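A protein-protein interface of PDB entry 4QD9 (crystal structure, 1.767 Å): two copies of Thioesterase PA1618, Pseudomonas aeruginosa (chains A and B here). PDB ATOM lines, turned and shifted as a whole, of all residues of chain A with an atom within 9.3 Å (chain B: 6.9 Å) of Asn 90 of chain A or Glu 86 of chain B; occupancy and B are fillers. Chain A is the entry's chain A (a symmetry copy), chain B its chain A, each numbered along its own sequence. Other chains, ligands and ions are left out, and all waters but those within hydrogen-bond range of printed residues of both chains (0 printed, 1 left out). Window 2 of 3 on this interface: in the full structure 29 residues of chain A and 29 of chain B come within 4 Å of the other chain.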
ATOM      1  N   GLY A  56      14.466  -7.777   5.814  1.00  0.00           N
ATOM      2  CA  GLY A  56      13.701  -8.407   4.754  1.00  0.00           C
ATOM      3  C   GLY A  56      14.561  -8.630   3.527  1.00  0.00           C
ATOM      4  O   GLY A  56      14.392  -9.608   2.798  1.00  0.00           O
ATOM      5  N   GLY A  57      15.509  -7.730   3.299  1.00  0.00           N
ATOM      6  CA  GLY A  57      16.420  -7.898   2.181  1.00  0.00           C
ATOM      7  C   GLY A  57      17.341  -9.084   2.372  1.00  0.00           C
ATOM      8  O   GLY A  57      17.761  -9.722   1.398  1.00  0.00           O
ATOM      9  N   SER A  59      16.521 -11.891   3.792  1.00  0.00           N
ATOM     10  CA  SER A  59      15.733 -13.042   3.354  1.00  0.00           C
ATOM     11  C   SER A  59      15.834 -13.172   1.844  1.00  0.00           C
ATOM     12  O   SER A  59      15.930 -14.286   1.313  1.00  0.00           O
ATOM     13  CB  SER A  59      14.259 -12.888   3.713  1.00  0.00           C
ATOM     14  OG  SER A  59      14.049 -13.055   5.091  1.00  0.00           O
ATOM     15  N   VAL A  60      15.831 -12.034   1.154  1.00  0.00           N
ATOM     16  CA  VAL A  60      15.911 -12.066  -0.302  1.00  0.00           C
ATOM     17  C   VAL A  60      17.305 -12.491  -0.765  1.00  0.00           C
ATOM     18  O   VAL A  60      17.427 -13.233  -1.746  1.00  0.00           O
ATOM     19  CB  VAL A  60      15.430 -10.745  -0.945  1.00  0.00           C
ATOM     20  CG1 VAL A  60      15.594 -10.786  -2.468  1.00  0.00           C
ATOM     21  CG2 VAL A  60      13.950 -10.510  -0.586  1.00  0.00           C
ATOM     22  N   ALA A  63      17.231 -16.188  -0.534  1.00  0.00           N
ATOM     23  CA  ALA A  63      16.394 -16.772  -1.586  1.00  0.00           C
ATOM     24  C   ALA A  63      17.068 -16.708  -2.957  1.00  0.00           C
ATOM     25  O   ALA A  63      17.034 -17.677  -3.734  1.00  0.00           O
ATOM     26  CB  ALA A  63      15.027 -16.093  -1.619  1.00  0.00           C
ATOM     27  N   GLU A  86      14.105 -11.238 -12.186  1.00  0.00           N
ATOM     28  CA  GLU A  86      13.036 -10.646 -11.354  1.00  0.00           C
ATOM     29  C   GLU A  86      12.945 -11.400 -10.032  1.00  0.00           C
ATOM     30  O   GLU A  86      13.120 -12.622  -9.982  1.00  0.00           O
ATOM     31  CB  GLU A  86      11.678 -10.727 -12.078  1.00  0.00           C
ATOM     32  CG  GLU A  86      10.688  -9.582 -11.741  1.00  0.00           C
ATOM     33  CD  GLU A  86       9.890  -9.782 -10.454  1.00  0.00           C
ATOM     34  OE1 GLU A  86       9.764 -10.933  -9.981  1.00  0.00           O
ATOM     35  OE2 GLU A  86       9.370  -8.769  -9.913  1.00  0.00           O
ATOM     36  N   VAL A  87      12.694 -10.685  -8.940  1.00  0.00           N
ATOM     37  CA  VAL A  87      12.503 -11.374  -7.661  1.00  0.00           C
ATOM     38  C   VAL A  87      11.382 -10.700  -6.890  1.00  0.00           C
ATOM     39  O   VAL A  87      11.192  -9.486  -6.985  1.00  0.00           O
ATOM     40  CB  VAL A  87      13.821 -11.461  -6.809  1.00  0.00           C
ATOM     41  CG1 VAL A  87      14.272 -10.083  -6.262  1.00  0.00           C
ATOM     42  CG2 VAL A  87      13.647 -12.465  -5.678  1.00  0.00           C
ATOM     43  N   ASN A  88      10.633 -11.487  -6.136  1.00  0.00           N
ATOM     44  CA  ASN A  88       9.596 -10.903  -5.290  1.00  0.00           C
ATOM     45  C   ASN A  88       9.431 -11.719  -4.015  1.00  0.00           C
ATOM     46  O   ASN A  88       9.792 -12.895  -3.972  1.00  0.00           O
ATOM     47  CB  ASN A  88       8.275 -10.704  -6.062  1.00  0.00           C
ATOM     48  CG  ASN A  88       7.748 -11.977  -6.683  1.00  0.00           C
ATOM     49  OD1 ASN A  88       7.849 -12.186  -7.903  1.00  0.00           O
ATOM     50  ND2 ASN A  88       7.182 -12.836  -5.864  1.00  0.00           N
ATOM     51  N   ALA A  89       8.946 -11.089  -2.952  1.00  0.00           N
ATOM     52  CA  ALA A  89       8.815 -11.803  -1.684  1.00  0.00           C
ATOM     53  C   ALA A  89       7.713 -11.188  -0.852  1.00  0.00           C
ATOM     54  O   ALA A  89       7.535  -9.971  -0.878  1.00  0.00           O
ATOM     55  CB  ALA A  89      10.150 -11.766  -0.896  1.00  0.00           C
ATOM     56  N   ASN A  90       6.969 -12.033  -0.135  1.00  0.00           N
ATOM     57  CA  ASN A  90       6.109 -11.564   0.951  1.00  0.00           C
ATOM     58  C   ASN A  90       6.774 -11.878   2.268  1.00  0.00           C
ATOM     59  O   ASN A  90       7.189 -13.008   2.507  1.00  0.00           O
ATOM     60  CB  ASN A  90       4.735 -12.238   0.915  1.00  0.00           C
ATOM     61  CG  ASN A  90       3.743 -11.491   0.068  1.00  0.00           C
ATOM     62  OD1 ASN A  90       2.944 -10.693   0.572  1.00  0.00           O
ATOM     63  ND2 ASN A  90       3.769 -11.751  -1.221  1.00  0.00           N
ATOM     64  N   HIS A  91       6.864 -10.869   3.128  1.00  0.00           N
ATOM     65  CA  HIS A  91       7.424 -11.016   4.459  1.00  0.00           C
ATOM     66  C   HIS A  91       6.284 -11.346   5.427  1.00  0.00           C
ATOM     67  O   HIS A  91       5.418 -10.514   5.678  1.00  0.00           O
ATOM     68  CB  HIS A  91       8.125  -9.709   4.851  1.00  0.00           C
ATOM     69  CG  HIS A  91       9.247  -9.329   3.931  1.00  0.00           C
ATOM     70  ND1 HIS A  91      10.276 -10.195   3.616  1.00  0.00           N
ATOM     71  CD2 HIS A  91       9.514  -8.174   3.277  1.00  0.00           C
ATOM     72  CE1 HIS A  91      11.122  -9.592   2.798  1.00  0.00           C
ATOM     73  NE2 HIS A  91      10.683  -8.366   2.574  1.00  0.00           N
ATOM     74  N   LEU A  92       6.282 -12.571   5.945  1.00  0.00           N
ATOM     75  CA  LEU A  92       5.121 -13.117   6.653  1.00  0.00           C
ATOM     76  C   LEU A  92       5.201 -12.960   8.165  1.00  0.00           C
ATOM     77  O   LEU A  92       4.216 -12.574   8.801  1.00  0.00           O
ATOM     78  CB  LEU A  92       4.981 -14.608   6.341  1.00  0.00           C
ATOM     79  CG  LEU A  92       4.986 -14.925   4.845  1.00  0.00           C
ATOM     80  CD1 LEU A  92       4.975 -16.433   4.655  1.00  0.00           C
ATOM     81  CD2 LEU A  92       3.772 -14.298   4.169  1.00  0.00           C
ATOM     82  N   ARG A  93       6.363 -13.295   8.721  1.00  0.00           N
ATOM     83  CA  ARG A  93       6.604 -13.261  10.164  1.00  0.00           C
ATOM     84  C   ARG A  93       8.005 -12.752  10.438  1.00  0.00           C
ATOM     85  O   ARG A  93       8.953 -13.082   9.715  1.00  0.00           O
ATOM     86  CB  ARG A  93       6.476 -14.663  10.775  1.00  0.00           C
ATOM     87  CG  ARG A  93       5.060 -15.210  10.803  1.00  0.00           C
ATOM     88  CD  ARG A  93       4.997 -16.572  11.490  1.00  0.00           C
ATOM     89  NE  ARG A  93       3.605 -16.977  11.712  1.00  0.00           N
ATOM     90  CZ  ARG A  93       2.862 -17.597  10.797  1.00  0.00           C
ATOM     91  NH1 ARG A  93       3.378 -17.891   9.608  1.00  0.00           N
ATOM     92  NH2 ARG A  93       1.606 -17.932  11.067  1.00  0.00           N
ATOM     93  N   GLY A  94       8.152 -11.967  11.500  1.00  0.00           N
ATOM     94  CA  GLY A  94       9.470 -11.499  11.882  1.00  0.00           C
ATOM     95  C   GLY A  94      10.271 -12.538  12.644  1.00  0.00           C
ATOM     96  O   GLY A  94       9.709 -13.399  13.333  1.00  0.00           O
ATOM     97  N   ILE A 118      10.551 -20.311  -3.436  1.00  0.00           N
ATOM     98  CA  ILE A 118      11.450 -20.424  -2.281  1.00  0.00           C
ATOM     99  C   ILE A 118      10.664 -20.132  -0.997  1.00  0.00           C
ATOM    100  O   ILE A 118      10.070 -19.060  -0.855  1.00  0.00           O
ATOM    101  CB  ILE A 118      12.681 -19.487  -2.381  1.00  0.00           C
ATOM    102  CG1 ILE A 118      13.449 -19.747  -3.681  1.00  0.00           C
ATOM    103  CG2 ILE A 118      13.646 -19.751  -1.212  1.00  0.00           C
ATOM    104  CD1 ILE A 118      13.232 -18.695  -4.733  1.00  0.00           C
ATOM    105  N   ARG A 119      10.649 -21.092  -0.074  1.00  0.00           N
ATOM    106  CA  ARG A 119       9.878 -20.961   1.162  1.00  0.00           C
ATOM    107  C   ARG A 119      10.855 -20.862   2.332  1.00  0.00           C
ATOM    108  O   ARG A 119      11.772 -21.682   2.441  1.00  0.00           O
ATOM    109  CB  ARG A 119       8.963 -22.171   1.369  1.00  0.00           C
ATOM    110  CG  ARG A 119       8.063 -22.546   0.191  1.00  0.00           C
ATOM    111  CD  ARG A 119       7.005 -21.507  -0.075  1.00  0.00           C
ATOM    112  NE  ARG A 119       6.105 -21.926  -1.151  1.00  0.00           N
ATOM    113  CZ  ARG A 119       4.920 -22.503  -0.963  1.00  0.00           C
ATOM    114  NH1 ARG A 119       4.464 -22.721   0.266  1.00  0.00           N
ATOM    115  NH2 ARG A 119       4.183 -22.847  -2.010  1.00  0.00           N
ATOM    116  N   LEU A 120      10.669 -19.854   3.189  1.00  0.00           N
ATOM    117  CA  LEU A 120      11.562 -19.626   4.319  1.00  0.00           C
ATOM    118  C   LEU A 120      10.781 -19.777   5.630  1.00  0.00           C
ATOM    119  O   LEU A 120       9.580 -19.452   5.700  1.00  0.00           O
ATOM    120  CB  LEU A 120      12.220 -18.237   4.255  1.00  0.00           C
ATOM    121  CG  LEU A 120      13.252 -17.953   3.152  1.00  0.00           C
ATOM    122  CD1 LEU A 120      12.573 -17.840   1.801  1.00  0.00           C
ATOM    123  CD2 LEU A 120      14.020 -16.678   3.450  1.00  0.00           C
ATOM    124  N   PRO A 127       6.132 -20.447   8.594  1.00  0.00           N
ATOM    125  CA  PRO A 127       6.494 -19.651   7.410  1.00  0.00           C
ATOM    126  C   PRO A 127       6.840 -18.209   7.775  1.00  0.00           C
ATOM    127  O   PRO A 127       6.053 -17.557   8.464  1.00  0.00           O
ATOM    128  CB  PRO A 127       5.205 -19.682   6.573  1.00  0.00           C
ATOM    129  CG  PRO A 127       4.599 -21.025   6.919  1.00  0.00           C
ATOM    130  CD  PRO A 127       4.852 -21.158   8.410  1.00  0.00           C
ATOM    131  N   SER A 128       7.996 -17.719   7.327  1.00  0.00           N
ATOM    132  CA  SER A 128       8.430 -16.367   7.676  1.00  0.00           C
ATOM    133  C   SER A 128       8.536 -15.482   6.443  1.00  0.00           C
ATOM    134  O   SER A 128       8.401 -14.262   6.527  1.00  0.00           O
ATOM    135  CB  SER A 128       9.773 -16.416   8.390  1.00  0.00           C
ATOM    136  OG  SER A 128      10.788 -16.954   7.546  1.00  0.00           O
ATOM    137  N   CYS A 129       8.790 -16.110   5.298  1.00  0.00           N
ATOM    138  CA  CYS A 129       8.884 -15.397   4.032  1.00  0.00           C
ATOM    139  C   CYS A 129       8.595 -16.376   2.897  1.00  0.00           C
ATOM    140  O   CYS A 129       8.924 -17.564   2.993  1.00  0.00           O
ATOM    141  CB  CYS A 129      10.287 -14.793   3.887  1.00  0.00           C
ATOM    142  SG  CYS A 129      10.573 -13.827   2.384  1.00  0.00           S
ATOM    143  N   ILE A 130       7.942 -15.898   1.842  1.00  0.00           N
ATOM    144  CA  ILE A 130       7.851 -16.683   0.617  1.00  0.00           C
ATOM    145  C   ILE A 130       8.366 -15.824  -0.517  1.00  0.00           C
ATOM    146  O   ILE A 130       7.997 -14.658  -0.619  1.00  0.00           O
ATOM    147  CB  ILE A 130       6.419 -17.183   0.323  1.00  0.00           C
ATOM    148  CG1 ILE A 130       6.378 -17.910  -1.034  1.00  0.00           C
ATOM    149  CG2 ILE A 130       5.405 -16.019   0.378  1.00  0.00           C
ATOM    150  CD1 ILE A 130       5.084 -18.651  -1.276  1.00  0.00           C
ATOM    151  N   ALA A 131       9.214 -16.401  -1.375  1.00  0.00           N
ATOM    152  CA  ALA A 131       9.807 -15.647  -2.477  1.00  0.00           C
ATOM    153  C   ALA A 131       9.571 -16.372  -3.792  1.00  0.00           C
ATOM    154  O   ALA A 131       9.398 -17.598  -3.806  1.00  0.00           O
ATOM    155  CB  ALA A 131      11.309 -15.440  -2.248  1.00  0.00           C
ATOM    156  N   ARG A 132       9.538 -15.619  -4.891  1.00  0.00           N
ATOM    157  CA  ARG A 132       9.552 -16.259  -6.216  1.00  0.00           C
ATOM    158  C   ARG A 132      10.626 -15.569  -7.040  1.00  0.00           C
ATOM    159  O   ARG A 132      10.751 -14.341  -7.007  1.00  0.00           O
ATOM    160  CB  ARG A 132       8.154 -16.234  -6.884  1.00  0.00           C
ATOM    161  CG  ARG A 132       8.015 -17.223  -8.080  1.00  0.00           C
ATOM    162  CD  ARG A 132       6.572 -17.368  -8.588  1.00  0.00           C
ATOM    163  NE  ARG A 132       6.152 -16.140  -9.264  1.00  0.00           N
ATOM    164  CZ  ARG A 132       5.314 -15.250  -8.746  1.00  0.00           C
ATOM    165  NH1 ARG A 132       4.760 -15.475  -7.556  1.00  0.00           N
ATOM    166  NH2 ARG A 132       5.036 -14.141  -9.418  1.00  0.00           N
ATOM    167  N   GLU B  64      15.410  -2.110   0.418  1.00  0.00           N
ATOM    168  CA  GLU B  64      14.560  -2.266   1.598  1.00  0.00           C
ATOM    169  C   GLU B  64      15.105  -1.469   2.801  1.00  0.00           C
ATOM    170  O   GLU B  64      14.324  -0.972   3.612  1.00  0.00           O
ATOM    171  CB  GLU B  64      14.321  -3.757   1.925  1.00  0.00           C
ATOM    172  CG  GLU B  64      13.369  -3.981   3.110  1.00  0.00           C
ATOM    173  CD  GLU B  64      12.556  -5.276   3.031  1.00  0.00           C
ATOM    174  OE1 GLU B  64      12.398  -5.875   1.927  1.00  0.00           O
ATOM    175  OE2 GLU B  64      12.067  -5.697   4.098  1.00  0.00           O
ATOM    176  N   VAL B  83       7.139  -2.239   9.131  1.00  0.00           N
ATOM    177  CA  VAL B  83       7.939  -3.390   8.730  1.00  0.00           C
ATOM    178  C   VAL B  83       7.642  -3.729   7.283  1.00  0.00           C
ATOM    179  O   VAL B  83       6.530  -3.505   6.798  1.00  0.00           O
ATOM    180  CB  VAL B  83       7.651  -4.612   9.598  1.00  0.00           C
ATOM    181  CG1 VAL B  83       8.244  -4.416  10.990  1.00  0.00           C
ATOM    182  CG2 VAL B  83       6.167  -4.846   9.676  1.00  0.00           C
ATOM    183  N   GLY B  84       8.638  -4.261   6.592  1.00  0.00           N
ATOM    184  CA  GLY B  84       8.426  -4.677   5.216  1.00  0.00           C
ATOM    185  C   GLY B  84       7.353  -5.736   5.112  1.00  0.00           C
ATOM    186  O   GLY B  84       7.330  -6.680   5.888  1.00  0.00           O
ATOM    187  N   LEU B  85       6.487  -5.597   4.109  1.00  0.00           N
ATOM    188  CA  LEU B  85       5.379  -6.512   3.898  1.00  0.00           C
ATOM    189  C   LEU B  85       5.545  -7.272   2.576  1.00  0.00           C
ATOM    190  O   LEU B  85       5.364  -8.498   2.521  1.00  0.00           O
ATOM    191  CB  LEU B  85       4.082  -5.716   3.892  1.00  0.00           C
ATOM    192  CG  LEU B  85       2.797  -6.493   3.651  1.00  0.00           C
ATOM    193  CD1 LEU B  85       2.595  -7.494   4.791  1.00  0.00           C
ATOM    194  CD2 LEU B  85       1.626  -5.517   3.559  1.00  0.00           C
ATOM    195  N   GLU B  86       5.891  -6.536   1.522  1.00  0.00           N
ATOM    196  CA  GLU B  86       6.122  -7.133   0.190  1.00  0.00           C
ATOM    197  C   GLU B  86       7.235  -6.372  -0.522  1.00  0.00           C
ATOM    198  O   GLU B  86       7.350  -5.149  -0.399  1.00  0.00           O
ATOM    199  CB  GLU B  86       4.839  -7.070  -0.663  1.00  0.00           C
ATOM    200  CG  GLU B  86       4.677  -8.222  -1.688  1.00  0.00           C
ATOM    201  CD  GLU B  86       5.430  -8.022  -3.001  1.00  0.00           C
ATOM    202  OE1 GLU B  86       5.774  -6.870  -3.343  1.00  0.00           O
ATOM    203  OE2 GLU B  86       5.668  -9.037  -3.710  1.00  0.00           O
ATOM    204  N   VAL B  87       8.083  -7.083  -1.257  1.00  0.00           N
ATOM    205  CA  VAL B  87       9.112  -6.389  -2.035  1.00  0.00           C
ATOM    206  C   VAL B  87       9.265  -7.069  -3.385  1.00  0.00           C
ATOM    207  O   VAL B  87       9.103  -8.286  -3.500  1.00  0.00           O
ATOM    208  CB  VAL B  87      10.487  -6.284  -1.280  1.00  0.00           C
ATOM    209  CG1 VAL B  87      11.195  -7.655  -1.135  1.00  0.00           C
ATOM    210  CG2 VAL B  87      11.390  -5.276  -1.977  1.00  0.00           C
ATOM    211  N   ASN B  88       9.566  -6.285  -4.407  1.00  0.00           N
ATOM    212  CA  ASN B  88       9.824  -6.875  -5.717  1.00  0.00           C
ATOM    213  C   ASN B  88      10.861  -6.053  -6.473  1.00  0.00           C
ATOM    214  O   ASN B  88      11.059  -4.874  -6.181  1.00  0.00           O
ATOM    215  CB  ASN B  88       8.520  -7.091  -6.512  1.00  0.00           C
ATOM    216  CG  ASN B  88       7.711  -5.827  -6.689  1.00  0.00           C
ATOM    217  OD1 ASN B  88       6.683  -5.623  -6.023  1.00  0.00           O
ATOM    218  ND2 ASN B  88       8.155  -4.969  -7.581  1.00  0.00           N
ATOM    219  N   ARG B 132      10.102  -2.157  -5.984  1.00  0.00           N
ATOM    220  CA  ARG B 132       8.937  -1.525  -5.347  1.00  0.00           C
ATOM    221  C   ARG B 132       8.728  -2.209  -4.007  1.00  0.00           C
ATOM    222  O   ARG B 132       8.828  -3.435  -3.906  1.00  0.00           O
ATOM    223  CB  ARG B 132       7.686  -1.567  -6.261  1.00  0.00           C
ATOM    224  CG  ARG B 132       6.558  -0.586  -5.821  1.00  0.00           C
ATOM    225  CD  ARG B 132       5.425  -0.458  -6.851  1.00  0.00           C
ATOM    226  NE  ARG B 132       4.642  -1.694  -6.894  1.00  0.00           N
ATOM    227  CZ  ARG B 132       4.709  -2.589  -7.872  1.00  0.00           C
ATOM    228  NH1 ARG B 132       5.491  -2.363  -8.925  1.00  0.00           N
ATOM    229  NH2 ARG B 132       3.996  -3.705  -7.791  1.00  0.00           N
ATOM    230  N   LEU B 133       8.496  -1.411  -2.963  1.00  0.00           N
ATOM    231  CA  LEU B 133       8.466  -1.914  -1.589  1.00  0.00           C
ATOM    232  C   LEU B 133       7.152  -1.505  -0.948  1.00  0.00           C
ATOM    233  O   LEU B 133       6.765  -0.338  -1.036  1.00  0.00           O
ATOM    234  CB  LEU B 133       9.596  -1.265  -0.787  1.00  0.00           C
ATOM    235  CG  LEU B 133       9.647  -1.573   0.715  1.00  0.00           C
ATOM    236  CD1 LEU B 133       9.868  -3.054   0.960  1.00  0.00           C
ATOM    237  CD2 LEU B 133      10.776  -0.761   1.373  1.00  0.00           C
ATOM    238  N   THR B 134       6.489  -2.457  -0.299  1.00  0.00           N
ATOM    239  CA  THR B 134       5.263  -2.184   0.455  1.00  0.00           C
ATOM    240  C   THR B 134       5.571  -2.416   1.919  1.00  0.00           C
ATOM    241  O   THR B 134       5.999  -3.499   2.294  1.00  0.00           O
ATOM    242  CB  THR B 134       4.152  -3.138   0.030  1.00  0.00           C
ATOM    243  OG1 THR B 134       3.973  -3.040  -1.389  1.00  0.00           O
ATOM    244  CG2 THR B 134       2.832  -2.800   0.732  1.00  0.00           C
ATOM    245  N   MET B 135       5.359  -1.387   2.738  1.00  0.00           N
ATOM    246  CA  MET B 135       5.598  -1.460   4.180  1.00  0.00           C
ATOM    247  C   MET B 135       4.255  -1.494   4.877  1.00  0.00           C
ATOM    248  O   MET B 135       3.318  -0.836   4.432  1.00  0.00           O
ATOM    249  CB  MET B 135       6.338  -0.208   4.658  1.00  0.00           C
ATOM    250  CG  MET B 135       7.662   0.070   3.965  1.00  0.00           C
ATOM    251  SD  MET B 135       8.879  -1.119   4.520  1.00  0.00           S
ATOM    252  CE  MET B 135       8.964  -0.750   6.279  1.00  0.00           C
ATOM    253  N   ALA B 136       4.150  -2.275   5.951  1.00  0.00           N
ATOM    254  CA  ALA B 136       2.965  -2.244   6.807  1.00  0.00           C
ATOM    255  C   ALA B 136       3.211  -1.248   7.933  1.00  0.00           C
ATOM    256  O   ALA B 136       4.313  -1.178   8.459  1.00  0.00           O
ATOM    257  CB  ALA B 136       2.691  -3.624   7.389  1.00  0.00           C
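Of the printed residues of chain B, Gly 56 of chain A touches Glu 64 (3.2 Å).
Of chain B, only Leu 85 and Glu 86 come within 4 Å of Asn 90 of chain A.
Of the printed residues of chain B, His 91 of chain A touches Glu 64, Gly 84, Leu 85 and Val 87.
Of the printed residues of chain A, Glu 64 of chain B touches Gly 56 (3.2 Å), Gly 57 (3.8 Å) and His 91 (3.1 Å).
Of chain A, only Asn 88, Ala 89 and Asn 90 come within 4 Å of Glu 86 of chain B.
Printed residues of chain A within 4 Å of Val 87 of chain B: Asn 88, Ala 89 and His 91.
No residue of chain A comes within 4 Å of Thr 134 of chain B.
The nearest residue of chain B that does not touch Asn 90 of chain A is Val 87 of chain B (5.2 Å).
OE1 of Glu 64 of chain B sits at hydrogen-bond distance from NE2 of His 91 of chain A, 3.1 Å away.
The backbone carbonyl oxygen (O) of Leu 85 of chain B sits at hydrogen-bond distance from the backbone NH (N) of His 91 of chain A, 2.9 Å away.
The backbone carbonyl oxygen of Val 87 of chain B is in hydrogen-bond range of the backbone NH of Ala 89 of chain A (2.9 Å).
Among the printed residues, pairs that only touch across the chains: Gly 56 of chain A with Glu 64 of chain B (3.2 Å), Gly 57 of chain A with Glu 64 of chain B (3.8 Å), Glu 86 of chain A with Asn 88 of chain B (3.9 Å), Val 87 of chain A with Asn 88 of chain B (3.2 Å), Asn 88 of chain A with Glu 86 of chain B (3.9 Å), Asn 88 of chain A with Val 87 of chain B (3.2 Å), Asn 88 of chain A with Asn 88 of chain B (3.6 Å), Ala 89 of chain A with Glu 86 of chain B (3.3 Å), Asn 90 of chain A with Leu 85 of chain B (3.5 Å), Asn 90 of chain A with Glu 86 of chain B (3.7 Å), His 91 of chain A with Gly 84 of chain B (3.3 Å) and His 91 of chain A with Val 87 of chain B (3.8 Å).
The backbone NH (N) of Gly 84 of chain B sits close to the side-chain sulfur (SD) of Met 135 of chain B (3.8 Å).
O of Thr 134 of chain B lies within hydrogen-bond range of N of Leu 85 of chain B, 2.8 Å away.
The side-chain carboxylate (OE1) of Glu 86 of chain B lies close to the side-chain amide oxygen (OD1) of Asn 88 of chain B (3.1 Å).
OD1 of Asn 88 of chain A lies close to OE1 of Glu 86 of chain A (3.1 Å).
The backbone carbonyl oxygen (O) of Asn 90 of chain A sits close to the side-chain sulfur (SG) of Cys 129 of chain A, at 3.5 Å.
N of Asn 90 of chain A lies within hydrogen-bond range of O of Ile 130 of chain A, 2.9 Å away.
Glu 86 of chain A touches Asn 88 of chain B, and with the chains exchanged Asn 88 of chain A touches Glu 86 of chain B.
Val 87 of chain A touches Asn 88 of chain B, and with the chains exchanged Asn 88 of chain A touches Val 87 of chain B.
Asn 88 of chain B touches its own counterpart, Asn 88 of chain A.
Positions printed for both chains: 86, 87, 88 and 132.
Hydrophobic or aromatic side chains of chain B within 4 Å of the printed part of chain A: Val 87.
Along chain B the printed residues that touch a printed residue of chain A span positions 64 to 88.
Printed residues of chain A that touch a printed residue of chain B: Gly 56, Gly 57, Glu 86, Val 87, Asn 88, Ala 89, Asn 90 and His 91.
Among the printed residues, 15 pairs touch across the chains.
Among the printed residues, no Asp or Glu carboxylate lies within 4 Å of a Lys or Arg side-chain nitrogen of the other chain.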
